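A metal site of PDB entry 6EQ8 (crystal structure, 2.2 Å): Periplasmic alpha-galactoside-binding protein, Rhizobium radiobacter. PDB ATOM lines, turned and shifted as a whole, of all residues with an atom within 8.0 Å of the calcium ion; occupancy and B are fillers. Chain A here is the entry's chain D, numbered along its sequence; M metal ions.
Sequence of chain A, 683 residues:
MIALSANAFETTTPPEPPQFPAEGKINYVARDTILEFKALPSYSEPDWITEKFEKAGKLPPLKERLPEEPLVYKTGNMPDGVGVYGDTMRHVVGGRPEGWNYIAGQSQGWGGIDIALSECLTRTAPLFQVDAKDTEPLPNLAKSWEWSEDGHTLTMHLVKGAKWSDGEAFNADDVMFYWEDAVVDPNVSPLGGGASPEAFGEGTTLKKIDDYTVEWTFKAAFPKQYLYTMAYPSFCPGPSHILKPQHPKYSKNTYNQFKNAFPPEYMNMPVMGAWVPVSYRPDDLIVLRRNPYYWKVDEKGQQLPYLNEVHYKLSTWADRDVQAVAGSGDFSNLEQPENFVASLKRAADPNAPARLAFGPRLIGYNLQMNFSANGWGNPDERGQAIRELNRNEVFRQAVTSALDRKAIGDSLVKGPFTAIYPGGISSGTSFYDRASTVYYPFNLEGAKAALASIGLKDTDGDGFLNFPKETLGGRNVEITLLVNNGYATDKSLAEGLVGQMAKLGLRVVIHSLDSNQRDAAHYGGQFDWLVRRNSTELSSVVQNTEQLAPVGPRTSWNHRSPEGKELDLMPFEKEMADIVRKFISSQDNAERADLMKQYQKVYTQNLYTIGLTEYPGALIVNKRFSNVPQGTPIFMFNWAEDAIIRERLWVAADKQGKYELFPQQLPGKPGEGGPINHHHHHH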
ATOM      1  N   LYS A 457      24.887 -16.294 -21.281  1.00  0.00           N
ATOM      2  CA  LYS A 457      26.015 -15.375 -21.343  1.00  0.00           C
ATOM      3  C   LYS A 457      25.601 -13.907 -21.485  1.00  0.00           C
ATOM      4  O   LYS A 457      24.540 -13.615 -22.027  1.00  0.00           O
ATOM      5  CB  LYS A 457      27.044 -15.786 -22.431  1.00  0.00           C
ATOM      6  CG  LYS A 457      26.571 -15.676 -23.884  1.00  0.00           C
ATOM      7  CD  LYS A 457      27.713 -15.989 -24.850  1.00  0.00           C
ATOM      8  CE  LYS A 457      27.498 -15.414 -26.229  1.00  0.00           C
ATOM      9  NZ  LYS A 457      28.694 -15.611 -27.101  1.00  0.00           N
ATOM     10  N   ASP A 458      26.428 -13.002 -20.966  1.00  0.00           N
ATOM     11  CA  ASP A 458      26.230 -11.564 -21.068  1.00  0.00           C
ATOM     12  C   ASP A 458      26.552 -11.095 -22.525  1.00  0.00           C
ATOM     13  O   ASP A 458      27.707 -10.981 -22.928  1.00  0.00           O
ATOM     14  CB  ASP A 458      27.089 -10.838 -20.011  1.00  0.00           C
ATOM     15  CG  ASP A 458      27.008  -9.321 -20.061  1.00  0.00           C
ATOM     16  OD1 ASP A 458      25.943  -8.804 -20.468  1.00  0.00           O
ATOM     17  OD2 ASP A 458      28.014  -8.657 -19.713  1.00  0.00           O
ATOM     18  N   THR A 459      25.486 -10.849 -23.298  1.00  0.00           N
ATOM     19  CA  THR A 459      25.551 -10.435 -24.699  1.00  0.00           C
ATOM     20  C   THR A 459      25.388  -8.907 -24.926  1.00  0.00           C
ATOM     21  O   THR A 459      25.566  -8.444 -26.056  1.00  0.00           O
ATOM     22  CB  THR A 459      24.544 -11.228 -25.563  1.00  0.00           C
ATOM     23  OG1 THR A 459      23.212 -10.894 -25.188  1.00  0.00           O
ATOM     24  CG2 THR A 459      24.737 -12.744 -25.497  1.00  0.00           C
ATOM     25  N   ASP A 460      25.055  -8.135 -23.861  1.00  0.00           N
ATOM     26  CA  ASP A 460      24.864  -6.680 -23.923  1.00  0.00           C
ATOM     27  C   ASP A 460      25.899  -5.876 -23.087  1.00  0.00           C
ATOM     28  O   ASP A 460      25.893  -4.634 -23.137  1.00  0.00           O
ATOM     29  CB  ASP A 460      23.423  -6.264 -23.565  1.00  0.00           C
ATOM     30  CG  ASP A 460      22.803  -7.012 -22.398  1.00  0.00           C
ATOM     31  OD2 ASP A 460      21.559  -7.171 -22.395  1.00  0.00           O
ATOM     32  N   GLY A 461      26.805  -6.574 -22.408  1.00  0.00           N
ATOM     33  CA  GLY A 461      27.866  -5.955 -21.608  1.00  0.00           C
ATOM     34  C   GLY A 461      27.469  -5.300 -20.292  1.00  0.00           C
ATOM     35  O   GLY A 461      28.116  -4.335 -19.861  1.00  0.00           O
ATOM     36  N   ASP A 462      26.438  -5.820 -19.596  1.00  0.00           N
ATOM     37  CA  ASP A 462      26.041  -5.249 -18.301  1.00  0.00           C
ATOM     38  C   ASP A 462      26.392  -6.183 -17.143  1.00  0.00           C
ATOM     39  O   ASP A 462      26.042  -5.893 -15.987  1.00  0.00           O
ATOM     40  CB  ASP A 462      24.570  -4.797 -18.280  1.00  0.00           C
ATOM     41  CG  ASP A 462      23.545  -5.914 -18.418  1.00  0.00           C
ATOM     42  OD1 ASP A 462      23.930  -7.023 -18.855  1.00  0.00           O
ATOM     43  OD2 ASP A 462      22.362  -5.659 -18.121  1.00  0.00           O
ATOM     44  N   GLY A 463      27.048  -7.301 -17.466  1.00  0.00           N
ATOM     45  CA  GLY A 463      27.437  -8.331 -16.509  1.00  0.00           C
ATOM     46  C   GLY A 463      26.344  -9.363 -16.285  1.00  0.00           C
ATOM     47  O   GLY A 463      26.647 -10.526 -15.975  1.00  0.00           O
ATOM     48  N   PHE A 464      25.063  -8.944 -16.424  1.00  0.00           N
ATOM     49  CA  PHE A 464      23.922  -9.831 -16.262  1.00  0.00           C
ATOM     50  C   PHE A 464      23.832 -10.768 -17.477  1.00  0.00           C
ATOM     51  O   PHE A 464      24.112 -10.359 -18.609  1.00  0.00           O
ATOM     52  CB  PHE A 464      22.623  -9.024 -16.052  1.00  0.00           C
ATOM     53  CG  PHE A 464      22.509  -8.327 -14.713  1.00  0.00           C
ATOM     54  CD1 PHE A 464      23.079  -7.081 -14.502  1.00  0.00           C
ATOM     55  CD2 PHE A 464      21.790  -8.905 -13.669  1.00  0.00           C
ATOM     56  CE1 PHE A 464      22.974  -6.439 -13.265  1.00  0.00           C
ATOM     57  CE2 PHE A 464      21.650  -8.241 -12.444  1.00  0.00           C
ATOM     58  CZ  PHE A 464      22.235  -7.015 -12.247  1.00  0.00           C
ATOM     59  N   LEU A 465      23.462 -12.004 -17.237  1.00  0.00           N
ATOM     60  CA  LEU A 465      23.325 -13.026 -18.274  1.00  0.00           C
ATOM     61  C   LEU A 465      22.039 -12.874 -19.086  1.00  0.00           C
ATOM     62  O   LEU A 465      20.980 -12.502 -18.562  1.00  0.00           O
ATOM     63  CB  LEU A 465      23.424 -14.447 -17.683  1.00  0.00           C
ATOM     64  CG  LEU A 465      24.636 -14.744 -16.796  1.00  0.00           C
ATOM     65  CD1 LEU A 465      24.450 -16.042 -16.088  1.00  0.00           C
ATOM     66  CD2 LEU A 465      25.945 -14.735 -17.587  1.00  0.00           C
ATOM     67  N   ASN A 466      22.136 -13.205 -20.364  1.00  0.00           N
ATOM     68  CA  ASN A 466      21.064 -13.114 -21.341  1.00  0.00           C
ATOM     69  C   ASN A 466      20.591 -14.461 -21.785  1.00  0.00           C
ATOM     70  O   ASN A 466      21.378 -15.410 -21.819  1.00  0.00           O
ATOM     71  CB  ASN A 466      21.575 -12.375 -22.582  1.00  0.00           C
ATOM     72  CG  ASN A 466      21.896 -10.916 -22.379  1.00  0.00           C
ATOM     73  OD1 ASN A 466      21.175 -10.021 -22.844  1.00  0.00           O
ATOM     74  ND2 ASN A 466      23.016 -10.651 -21.745  1.00  0.00           N
ATOM     75  N   PHE A 467      19.327 -14.534 -22.209  1.00  0.00           N
ATOM     76  CA  PHE A 467      18.780 -15.727 -22.843  1.00  0.00           C
ATOM     77  C   PHE A 467      19.445 -15.857 -24.237  1.00  0.00           C
ATOM     78  O   PHE A 467      19.829 -14.809 -24.789  1.00  0.00           O
ATOM     79  CB  PHE A 467      17.276 -15.570 -23.040  1.00  0.00           C
ATOM     80  CG  PHE A 467      16.481 -15.874 -21.791  1.00  0.00           C
ATOM     81  CD1 PHE A 467      16.420 -17.172 -21.288  1.00  0.00           C
ATOM     82  CD2 PHE A 467      15.799 -14.864 -21.130  1.00  0.00           C
ATOM     83  CE1 PHE A 467      15.674 -17.452 -20.140  1.00  0.00           C
ATOM     84  CE2 PHE A 467      15.055 -15.153 -19.980  1.00  0.00           C
ATOM     85  CZ  PHE A 467      14.996 -16.444 -19.501  1.00  0.00           C
ATOM     86  N   GLY A 474      16.986 -12.704 -27.012  1.00  0.00           N
ATOM     87  CA  GLY A 474      18.268 -12.680 -26.319  1.00  0.00           C
ATOM     88  C   GLY A 474      18.379 -11.688 -25.177  1.00  0.00           C
ATOM     89  O   GLY A 474      19.486 -11.285 -24.836  1.00  0.00           O
ATOM     90  N   ARG A 475      17.245 -11.269 -24.598  1.00  0.00           N
ATOM     91  CA  ARG A 475      17.225 -10.297 -23.508  1.00  0.00           C
ATOM     92  C   ARG A 475      17.781 -10.907 -22.198  1.00  0.00           C
ATOM     93  O   ARG A 475      17.844 -12.151 -22.085  1.00  0.00           O
ATOM     94  CB  ARG A 475      15.776  -9.805 -23.316  1.00  0.00           C
ATOM     95  CG  ARG A 475      15.608  -8.547 -22.471  1.00  0.00           C
ATOM     96  CD  ARG A 475      14.170  -8.280 -22.021  1.00  0.00           C
ATOM     97  NE  ARG A 475      13.428  -9.460 -21.600  1.00  0.00           N
ATOM     98  CZ  ARG A 475      12.540 -10.103 -22.353  1.00  0.00           C
ATOM     99  NH1 ARG A 475      12.289  -9.698 -23.593  1.00  0.00           N
ATOM    100  NH2 ARG A 475      11.902 -11.164 -21.878  1.00  0.00           N
ATOM    101  N   ASN A 476      18.202 -10.042 -21.226  1.00  0.00           N
ATOM    102  CA  ASN A 476      18.679 -10.479 -19.904  1.00  0.00           C
ATOM    103  C   ASN A 476      17.638 -11.360 -19.214  1.00  0.00           C
ATOM    104  O   ASN A 476      16.433 -11.090 -19.332  1.00  0.00           O
ATOM    105  CB  ASN A 476      18.933  -9.288 -18.962  1.00  0.00           C
ATOM    106  CG  ASN A 476      20.240  -8.588 -19.112  1.00  0.00           C
ATOM    107  OD1 ASN A 476      21.243  -9.144 -19.570  1.00  0.00           O
ATOM    108  ND2 ASN A 476      20.267  -7.365 -18.654  1.00  0.00           N
ATOM    109  N   VAL A 477      18.121 -12.374 -18.459  1.00  0.00           N
ATOM    110  CA  VAL A 477      17.264 -13.259 -17.656  1.00  0.00           C
ATOM    111  C   VAL A 477      16.713 -12.441 -16.451  1.00  0.00           C
ATOM    112  O   VAL A 477      17.493 -11.811 -15.735  1.00  0.00           O
ATOM    113  CB  VAL A 477      18.000 -14.565 -17.215  1.00  0.00           C
ATOM    114  CG1 VAL A 477      17.129 -15.410 -16.277  1.00  0.00           C
ATOM    115  CG2 VAL A 477      18.441 -15.393 -18.435  1.00  0.00           C
ATOM    116  N   GLY A 505      24.903 -12.949 -11.820  1.00  0.00           N
ATOM    117  CA  GLY A 505      24.525 -12.377 -13.105  1.00  0.00           C
ATOM    118  C   GLY A 505      23.070 -12.561 -13.438  1.00  0.00           C
ATOM    119  O   GLY A 505      22.701 -12.474 -14.614  1.00  0.00           O
HETATM  120 CA    CA M   1      23.491  -8.765 -20.181  1.00  0.00          CA
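The side-chain amide oxygen of Asn 476 sits close to the side-chain carboxylate of Asp 460, 3.5 Å away.
N of Gly 461 sits close to OD1 of Asp 458, 3.1 Å away.
The side-chain carboxylate (OD2) of Asp 458 lies within hydrogen-bond range of the backbone NH (N) of Gly 463, at 2.8 Å.
The side-chain carboxylate (OD2) of Asp 460 lies close to the side-chain amide oxygen (OD1) of Asn 466, at 2.9 Å.
The side-chain hydroxyl of Thr 459 sits close to the side-chain amide oxygen of Asn 466 (3.2 Å).
The backbone carbonyl oxygen (O) of Lys 457 sits at hydrogen-bond distance from the backbone NH (N) of Asn 466 (3.0 Å).
OD1 of Asn 466 lies close to O of Gly 474 (2.9 Å).
The calcium ion is bound by the side-chain carboxylate (OD1) of Asp 462 (2.2 Å), the backbone carbonyl oxygen (O) of Phe 464 (2.3 Å), the side-chain amide oxygen (OD1) of Asn 476 (2.4 Å), the side-chain carboxylate (OD1) of Asp 458 (2.5 Å) and the side-chain amide nitrogen (ND2) of Asn 466 (2.5 Å).
The calcium ion has five donor atoms within binding distance.
CG of Asp 460 touches the calcium ion, 2.9 Å away.
Of the 16 residues printed, 6 come within 4 Å of the calcium ion.
The nearest printed residue that does not touch the calcium ion is Thr 459 (4.2 Å).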
